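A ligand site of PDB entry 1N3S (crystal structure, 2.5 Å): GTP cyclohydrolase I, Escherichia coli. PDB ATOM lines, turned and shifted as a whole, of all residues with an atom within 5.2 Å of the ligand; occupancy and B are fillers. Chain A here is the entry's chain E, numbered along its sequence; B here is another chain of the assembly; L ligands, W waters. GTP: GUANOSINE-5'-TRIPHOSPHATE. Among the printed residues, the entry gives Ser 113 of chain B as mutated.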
ATOM      1  N   LYS A  85      22.887  13.663  16.191  1.00  0.00           N
ATOM      2  CA  LYS A  85      21.544  13.444  15.684  1.00  0.00           C
ATOM      3  C   LYS A  85      21.650  12.812  14.300  1.00  0.00           C
ATOM      4  O   LYS A  85      21.776  13.514  13.302  1.00  0.00           O
ATOM      5  CB  LYS A  85      20.781  14.779  15.642  1.00  0.00           C
ATOM      6  CG  LYS A  85      20.620  15.414  17.025  1.00  0.00           C
ATOM      7  CD  LYS A  85      20.149  16.866  16.974  1.00  0.00           C
ATOM      8  CE  LYS A  85      20.057  17.435  18.388  1.00  0.00           C
ATOM      9  NZ  LYS A  85      19.698  18.884  18.418  1.00  0.00           N
ATOM     10  N   THR A  87      20.896  11.022  10.817  1.00  0.00           N
ATOM     11  CA  THR A  87      19.918  11.066   9.741  1.00  0.00           C
ATOM     12  C   THR A  87      20.294  10.082   8.644  1.00  0.00           C
ATOM     13  O   THR A  87      21.397  10.159   8.090  1.00  0.00           O
ATOM     14  CB  THR A  87      19.773  12.480   9.108  1.00  0.00           C
ATOM     15  OG1 THR A  87      21.038  12.933   8.599  1.00  0.00           O
ATOM     16  CG2 THR A  87      19.215  13.486  10.126  1.00  0.00           C
ATOM     17  N   TYR A 125      32.096   1.618   4.280  1.00  0.00           N
ATOM     18  CA  TYR A 125      30.908   0.791   4.364  1.00  0.00           C
ATOM     19  C   TYR A 125      30.242   0.603   2.998  1.00  0.00           C
ATOM     20  O   TYR A 125      30.519   1.358   2.060  1.00  0.00           O
ATOM     21  CB  TYR A 125      29.905   1.332   5.397  1.00  0.00           C
ATOM     22  CG  TYR A 125      29.079   2.534   4.997  1.00  0.00           C
ATOM     23  CD1 TYR A 125      29.620   3.840   5.044  1.00  0.00           C
ATOM     24  CD2 TYR A 125      27.738   2.389   4.592  1.00  0.00           C
ATOM     25  CE1 TYR A 125      28.832   4.977   4.702  1.00  0.00           C
ATOM     26  CE2 TYR A 125      26.944   3.515   4.243  1.00  0.00           C
ATOM     27  CZ  TYR A 125      27.505   4.799   4.308  1.00  0.00           C
ATOM     28  OH  TYR A 125      26.750   5.909   3.949  1.00  0.00           O
ATOM     29  N   VAL A 131      21.743   4.784   3.712  1.00  0.00           N
ATOM     30  CA  VAL A 131      22.963   5.544   3.480  1.00  0.00           C
ATOM     31  C   VAL A 131      22.982   6.551   4.639  1.00  0.00           C
ATOM     32  O   VAL A 131      22.011   7.273   4.839  1.00  0.00           O
ATOM     33  CB  VAL A 131      22.907   6.336   2.106  1.00  0.00           C
ATOM     34  CG1 VAL A 131      24.100   7.262   1.945  1.00  0.00           C
ATOM     35  CG2 VAL A 131      22.864   5.372   0.928  1.00  0.00           C
ATOM     36  N   ILE A 132      24.079   6.584   5.384  1.00  0.00           N
ATOM     37  CA  ILE A 132      24.212   7.522   6.505  1.00  0.00           C
ATOM     38  C   ILE A 132      24.754   8.845   5.974  1.00  0.00           C
ATOM     39  O   ILE A 132      25.432   8.868   4.931  1.00  0.00           O
ATOM     40  CB  ILE A 132      25.116   6.934   7.671  1.00  0.00           C
ATOM     41  CG1 ILE A 132      25.045   7.793   8.932  1.00  0.00           C
ATOM     42  CG2 ILE A 132      26.543   6.718   7.208  1.00  0.00           C
ATOM     43  CD1 ILE A 132      25.649   7.130  10.171  1.00  0.00           C
ATOM     44  N   GLY A 133      24.407   9.918   6.680  1.00  0.00           N
ATOM     45  CA  GLY A 133      24.849  11.259   6.336  1.00  0.00           C
ATOM     46  C   GLY A 133      26.335  11.290   6.610  1.00  0.00           C
ATOM     47  O   GLY A 133      26.767  10.762   7.633  1.00  0.00           O
ATOM     48  N   LEU A 134      27.107  11.873   5.691  1.00  0.00           N
ATOM     49  CA  LEU A 134      28.565  11.931   5.779  1.00  0.00           C
ATOM     50  C   LEU A 134      29.224  12.472   7.036  1.00  0.00           C
ATOM     51  O   LEU A 134      30.120  11.829   7.600  1.00  0.00           O
ATOM     52  CB  LEU A 134      29.145  12.612   4.543  1.00  0.00           C
ATOM     53  CG  LEU A 134      28.987  11.838   3.232  1.00  0.00           C
ATOM     54  CD1 LEU A 134      29.407  12.697   2.062  1.00  0.00           C
ATOM     55  CD2 LEU A 134      29.736  10.523   3.268  1.00  0.00           C
ATOM     56  N   SER A 135      28.788  13.656   7.490  1.00  0.00           N
ATOM     57  CA  SER A 135      29.353  14.262   8.697  1.00  0.00           C
ATOM     58  C   SER A 135      29.028  13.457   9.961  1.00  0.00           C
ATOM     59  O   SER A 135      29.756  13.547  10.958  1.00  0.00           O
ATOM     60  CB  SER A 135      28.900  15.713   8.842  1.00  0.00           C
ATOM     61  OG  SER A 135      27.494  15.801   8.980  1.00  0.00           O
ATOM     62  N   LYS A 136      27.962  12.647   9.902  1.00  0.00           N
ATOM     63  CA  LYS A 136      27.567  11.822  11.038  1.00  0.00           C
ATOM     64  C   LYS A 136      28.581  10.713  11.336  1.00  0.00           C
ATOM     65  O   LYS A 136      28.662  10.248  12.461  1.00  0.00           O
ATOM     66  CB  LYS A 136      26.144  11.245  10.865  1.00  0.00           C
ATOM     67  CG  LYS A 136      25.023  12.304  10.721  1.00  0.00           C
ATOM     68  CD  LYS A 136      25.194  13.503  11.691  1.00  0.00           C
ATOM     69  CE  LYS A 136      24.061  14.507  11.620  1.00  0.00           C
ATOM     70  NZ  LYS A 136      23.659  14.911  10.242  1.00  0.00           N
ATOM     71  N   ARG A 139      31.248  12.636  13.224  1.00  0.00           N
ATOM     72  CA  ARG A 139      30.709  12.913  14.553  1.00  0.00           C
ATOM     73  C   ARG A 139      30.647  11.674  15.454  1.00  0.00           C
ATOM     74  O   ARG A 139      30.819  11.792  16.668  1.00  0.00           O
ATOM     75  CB  ARG A 139      29.352  13.590  14.457  1.00  0.00           C
ATOM     76  CG  ARG A 139      29.393  14.944  13.796  1.00  0.00           C
ATOM     77  CD  ARG A 139      28.090  15.698  13.873  1.00  0.00           C
ATOM     78  NE  ARG A 139      28.338  17.001  14.492  1.00  0.00           N
ATOM     79  CZ  ARG A 139      28.045  18.177  13.938  1.00  0.00           C
ATOM     80  NH1 ARG A 139      27.487  18.222  12.740  1.00  0.00           N
ATOM     81  NH2 ARG A 139      28.353  19.295  14.564  1.00  0.00           N
ATOM     82  N   CYS B 110      26.452  20.624  -2.560  1.00  0.00           N
ATOM     83  CA  CYS B 110      25.660  19.674  -1.759  1.00  0.00           C
ATOM     84  C   CYS B 110      24.206  20.156  -1.698  1.00  0.00           C
ATOM     85  O   CYS B 110      23.974  21.334  -1.457  1.00  0.00           O
ATOM     86  CB  CYS B 110      26.241  19.489  -0.349  1.00  0.00           C
ATOM     87  SG  CYS B 110      25.962  20.849   0.822  1.00  0.00           S
ATOM     88  N   HIS B 112      22.040  19.437   0.500  1.00  0.00           N
ATOM     89  CA  HIS B 112      21.638  19.552   1.878  1.00  0.00           C
ATOM     90  C   HIS B 112      21.832  20.962   2.431  1.00  0.00           C
ATOM     91  O   HIS B 112      21.038  21.434   3.246  1.00  0.00           O
ATOM     92  CB  HIS B 112      22.329  18.444   2.707  1.00  0.00           C
ATOM     93  CG  HIS B 112      23.283  18.925   3.771  1.00  0.00           C
ATOM     94  ND1 HIS B 112      24.643  19.018   3.558  1.00  0.00           N
ATOM     95  CD2 HIS B 112      23.081  19.256   5.059  1.00  0.00           C
ATOM     96  CE1 HIS B 112      25.232  19.379   4.692  1.00  0.00           C
ATOM     97  NE2 HIS B 112      24.308  19.527   5.619  1.00  0.00           N
ATOM     98  N   SER B 113      22.847  21.666   1.920  1.00  0.00           N
ATOM     99  CA  SER B 113      23.177  23.003   2.405  1.00  0.00           C
ATOM    100  C   SER B 113      23.583  24.035   1.357  1.00  0.00           C
ATOM    101  O   SER B 113      23.915  25.190   1.701  1.00  0.00           O
ATOM    102  CB  SER B 113      24.306  22.882   3.436  1.00  0.00           C
ATOM    103  OG  SER B 113      23.833  22.391   4.685  1.00  0.00           O
ATOM    104  N   GLN B 149      23.651  18.225  -5.514  1.00  0.00           N
ATOM    105  CA  GLN B 149      23.961  16.800  -5.387  1.00  0.00           C
ATOM    106  C   GLN B 149      24.147  16.111  -4.047  1.00  0.00           C
ATOM    107  O   GLN B 149      24.260  16.738  -2.985  1.00  0.00           O
ATOM    108  CB  GLN B 149      25.187  16.466  -6.259  1.00  0.00           C
ATOM    109  CG  GLN B 149      24.967  16.430  -7.763  1.00  0.00           C
ATOM    110  CD  GLN B 149      24.194  15.198  -8.250  1.00  0.00           C
ATOM    111  OE1 GLN B 149      23.863  14.308  -7.479  1.00  0.00           O
ATOM    112  NE2 GLN B 149      23.940  15.139  -9.546  1.00  0.00           N
ATOM    113  N   VAL B 150      24.150  14.781  -4.155  1.00  0.00           N
ATOM    114  CA  VAL B 150      24.385  13.808  -3.092  1.00  0.00           C
ATOM    115  C   VAL B 150      25.460  12.952  -3.791  1.00  0.00           C
ATOM    116  O   VAL B 150      25.198  12.378  -4.865  1.00  0.00           O
ATOM    117  CB  VAL B 150      23.121  12.912  -2.776  1.00  0.00           C
ATOM    118  CG1 VAL B 150      23.473  11.759  -1.813  1.00  0.00           C
ATOM    119  CG2 VAL B 150      22.025  13.747  -2.159  1.00  0.00           C
ATOM    120  N   GLN B 151      26.653  12.869  -3.189  1.00  0.00           N
ATOM    121  CA  GLN B 151      27.811  12.143  -3.740  1.00  0.00           C
ATOM    122  C   GLN B 151      27.583  10.729  -4.224  1.00  0.00           C
ATOM    123  O   GLN B 151      28.085  10.348  -5.283  1.00  0.00           O
ATOM    124  CB  GLN B 151      28.994  12.151  -2.760  1.00  0.00           C
ATOM    125  CG  GLN B 151      30.327  12.267  -3.477  1.00  0.00           C
ATOM    126  CD  GLN B 151      31.512  12.206  -2.551  1.00  0.00           C
ATOM    127  OE1 GLN B 151      31.571  12.897  -1.528  1.00  0.00           O
ATOM    128  NE2 GLN B 151      32.484  11.373  -2.903  1.00  0.00           N
ATOM    129  N   GLU B 152      26.777   9.973  -3.473  1.00  0.00           N
ATOM    130  CA  GLU B 152      26.468   8.582  -3.796  1.00  0.00           C
ATOM    131  C   GLU B 152      25.587   8.428  -5.030  1.00  0.00           C
ATOM    132  O   GLU B 152      25.771   7.498  -5.822  1.00  0.00           O
ATOM    133  CB  GLU B 152      25.826   7.892  -2.591  1.00  0.00           C
ATOM    134  CG  GLU B 152      26.812   7.613  -1.453  1.00  0.00           C
ATOM    135  CD  GLU B 152      26.805   8.649  -0.332  1.00  0.00           C
ATOM    136  OE1 GLU B 152      26.576   9.843  -0.580  1.00  0.00           O
ATOM    137  OE2 GLU B 152      27.056   8.255   0.822  1.00  0.00           O
ATOM    138  N   HIS B 179      33.653  17.907   1.173  1.00  0.00           N
ATOM    139  CA  HIS B 179      32.411  18.652   1.329  1.00  0.00           C
ATOM    140  C   HIS B 179      32.746  19.784   2.273  1.00  0.00           C
ATOM    141  O   HIS B 179      33.282  19.540   3.351  1.00  0.00           O
ATOM    142  CB  HIS B 179      31.308  17.774   1.952  1.00  0.00           C
ATOM    143  CG  HIS B 179      30.825  16.681   1.068  1.00  0.00           C
ATOM    144  ND1 HIS B 179      29.501  16.581   0.678  1.00  0.00           N
ATOM    145  CD2 HIS B 179      31.474  15.667   0.452  1.00  0.00           C
ATOM    146  CE1 HIS B 179      29.369  15.550  -0.136  1.00  0.00           C
ATOM    147  NE2 HIS B 179      30.548  14.981  -0.282  1.00  0.00           N
ATOM    148  N   CYS B 181      30.676  21.565   3.834  1.00  0.00           N
ATOM    149  CA  CYS B 181      29.653  21.575   4.888  1.00  0.00           C
ATOM    150  C   CYS B 181      30.150  20.651   6.003  1.00  0.00           C
ATOM    151  O   CYS B 181      29.587  20.642   7.114  1.00  0.00           O
ATOM    152  CB  CYS B 181      28.329  21.085   4.339  1.00  0.00           C
ATOM    153  SG  CYS B 181      28.400  19.430   3.579  1.00  0.00           S
ATOM    154  N   VAL B 182      31.196  19.877   5.685  1.00  0.00           N
ATOM    155  CA  VAL B 182      31.851  18.964   6.618  1.00  0.00           C
ATOM    156  C   VAL B 182      33.144  19.619   7.089  1.00  0.00           C
ATOM    157  O   VAL B 182      33.507  19.513   8.268  1.00  0.00           O
ATOM    158  CB  VAL B 182      32.185  17.591   5.951  1.00  0.00           C
ATOM    159  CG1 VAL B 182      33.066  16.705   6.872  1.00  0.00           C
ATOM    160  CG2 VAL B 182      30.918  16.849   5.615  1.00  0.00           C
ATOM    161  N   ARG B 185      32.363  23.984   8.445  1.00  0.00           N
ATOM    162  CA  ARG B 185      31.153  24.159   9.247  1.00  0.00           C
ATOM    163  C   ARG B 185      30.858  22.839   9.998  1.00  0.00           C
ATOM    164  O   ARG B 185      31.417  21.786   9.669  1.00  0.00           O
ATOM    165  CB  ARG B 185      30.012  24.447   8.268  1.00  0.00           C
ATOM    166  CG  ARG B 185      28.774  25.043   8.852  1.00  0.00           C
ATOM    167  CD  ARG B 185      27.569  24.584   8.065  1.00  0.00           C
ATOM    168  NE  ARG B 185      27.384  23.130   8.080  1.00  0.00           N
ATOM    169  CZ  ARG B 185      26.773  22.444   9.036  1.00  0.00           C
ATOM    170  NH1 ARG B 185      26.285  23.039  10.106  1.00  0.00           N
ATOM    171  NH2 ARG B 185      26.602  21.137   8.886  1.00  0.00           N
ATOM    172  N   GLY B 186      29.995  22.920  11.010  1.00  0.00           N
ATOM    173  CA  GLY B 186      29.595  21.759  11.809  1.00  0.00           C
ATOM    174  C   GLY B 186      30.697  21.059  12.565  1.00  0.00           C
ATOM    175  O   GLY B 186      31.228  21.594  13.540  1.00  0.00           O
ATOM    176  N   ILE B 187      31.078  19.880  12.079  1.00  0.00           N
ATOM    177  CA  ILE B 187      32.147  19.080  12.679  1.00  0.00           C
ATOM    178  C   ILE B 187      33.534  19.703  12.459  1.00  0.00           C
ATOM    179  O   ILE B 187      34.469  19.457  13.226  1.00  0.00           O
ATOM    180  CB  ILE B 187      32.061  17.586  12.181  1.00  0.00           C
ATOM    181  CG1 ILE B 187      33.083  16.683  12.892  1.00  0.00           C
ATOM    182  CG2 ILE B 187      32.209  17.512  10.671  1.00  0.00           C
ATOM    183  CD1 ILE B 187      32.874  16.517  14.389  1.00  0.00           C
HETATM  184  PG  GTP L   1      26.035  18.468  10.277  1.00  0.00           P
HETATM  185  O1G GTP L   1      25.906  19.607  11.281  1.00  0.00           O
HETATM  186  O2G GTP L   1      25.763  17.077  10.820  1.00  0.00           O
HETATM  187  O3G GTP L   1      27.321  18.601   9.625  1.00  0.00           O
HETATM  188  O3B GTP L   1      24.911  18.805   9.155  1.00  0.00           O
HETATM  189  PB  GTP L   1      23.384  19.341   9.393  1.00  0.00           P
HETATM  190  O1B GTP L   1      23.447  20.431  10.466  1.00  0.00           O
HETATM  191  O2B GTP L   1      22.847  19.790   8.128  1.00  0.00           O
HETATM  192  O3A GTP L   1      22.659  18.067   9.925  1.00  0.00           O
HETATM  193  PA  GTP L   1      21.427  17.177   9.360  1.00  0.00           P
HETATM  194  O1A GTP L   1      20.838  16.426  10.449  1.00  0.00           O
HETATM  195  O2A GTP L   1      20.524  18.148   8.608  1.00  0.00           O
HETATM  196  O5' GTP L   1      22.107  16.040   8.356  1.00  0.00           O
HETATM  197  C5' GTP L   1      22.756  16.612   7.142  1.00  0.00           C
HETATM  198  C4' GTP L   1      23.647  15.326   6.843  1.00  0.00           C
HETATM  199  O4' GTP L   1      23.694  14.880   5.451  1.00  0.00           O
HETATM  200  C3' GTP L   1      25.046  15.387   7.257  1.00  0.00           C
HETATM  201  O3' GTP L   1      25.479  14.242   7.949  1.00  0.00           O
HETATM  202  C2' GTP L   1      25.884  15.703   6.004  1.00  0.00           C
HETATM  203  O2' GTP L   1      27.170  15.437   6.137  1.00  0.00           O
HETATM  204  C1' GTP L   1      25.034  14.620   5.081  1.00  0.00           C
HETATM  205  N9  GTP L   1      25.306  14.843   3.615  1.00  0.00           N
HETATM  206  C8  GTP L   1      25.415  16.072   2.991  1.00  0.00           C
HETATM  207  N7  GTP L   1      25.669  15.645   1.738  1.00  0.00           N
HETATM  208  C5  GTP L   1      25.724  14.264   1.575  1.00  0.00           C
HETATM  209  C6  GTP L   1      25.972  13.586   0.532  1.00  0.00           C
HETATM  210  O6  GTP L   1      26.228  13.772  -0.674  1.00  0.00           O
HETATM  211  N1  GTP L   1      25.925  12.070   0.812  1.00  0.00           N
HETATM  212  C2  GTP L   1      25.671  11.741   2.042  1.00  0.00           C
HETATM  213  N2  GTP L   1      25.646  10.279   2.318  1.00  0.00           N
HETATM  214  N3  GTP L   1      25.426  12.466   3.142  1.00  0.00           N
HETATM  215  C4  GTP L   1      25.489  13.781   2.784  1.00  0.00           C
HETATM  216  O   HOH W   1      29.683  19.217   9.367  1.00  0.00           O
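An oxygen (O2') of the ligand lies within hydrogen-bond range of the backbone NH (N) of Ser 135, 2.8 Å away.
The guanidinium group (NH2) of Arg 185 of chain B lies within salt-bridge range of an oxygen (O3G) of the ligand, at 2.7 Å.
N3 of the ligand is in hydrogen-bond range of N of Leu 134 (3.1 Å).
The guanidinium group (NH1) of Arg 139 lies within salt-bridge range of an oxygen (O1G) of the ligand, at 2.6 Å.
A nitrogen (N2) of the ligand sits at hydrogen-bond distance from the backbone carbonyl oxygen (O) of Ile 132, at 3.0 Å.
NZ of Lys 136 is in salt-bridge range of O2G of the ligand (3.1 Å).
NE2 of His 112 of chain B sits at hydrogen-bond distance from O2B of the ligand (2.9 Å).
The side-chain carboxylate of Glu 152 of chain B lies within hydrogen-bond range of a nitrogen (N1) of the ligand.
The side-chain hydroxyl of Thr 87 sits at hydrogen-bond distance from an oxygen (O5') of the ligand.
The side-chain hydroxyl of Ser 135 lies within hydrogen-bond range of an oxygen (O3') of the ligand, 2.7 Å away.
O6 of the ligand sits at hydrogen-bond distance from N of Gln 151 of chain B, at 2.7 Å.
The side-chain amide oxygen of Gln 151 of chain B is in hydrogen-bond range of a ring nitrogen (NE2) of His 179 of chain B (2.6 Å).
A ring nitrogen (ND1) of His 112 of chain B lies within hydrogen-bond range of the side-chain sulfur (SG) of Cys 110 of chain B.
NE of Arg 185 of chain B is in hydrogen-bond range of O of Cys 181 of chain B (3.5 Å).
N of Gly 133 sits at hydrogen-bond distance from O of Thr 87 (3.3 Å).
The side-chain sulfur (SG) of Cys 181 of chain B lies close to a ring nitrogen (ND1) of His 112 of chain B, at 3.8 Å.
The backbone NH (N) of Ile 132 lies within hydrogen-bond range of the side-chain hydroxyl (OH) of Tyr 125, 3.1 Å away.
Merely in contact with the ligand: Val 150 of chain B, Gly 133, Val 131, His 179 of chain B and Cys 181 of chain B.
Water W1 lies within hydrogen-bond range of O3G of the ligand (2.5 Å), O of Cys 181 of chain B (2.7 Å), O of Arg 185 of chain B (3.1 Å) and N of Ile 187 of chain B (3.1 Å).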
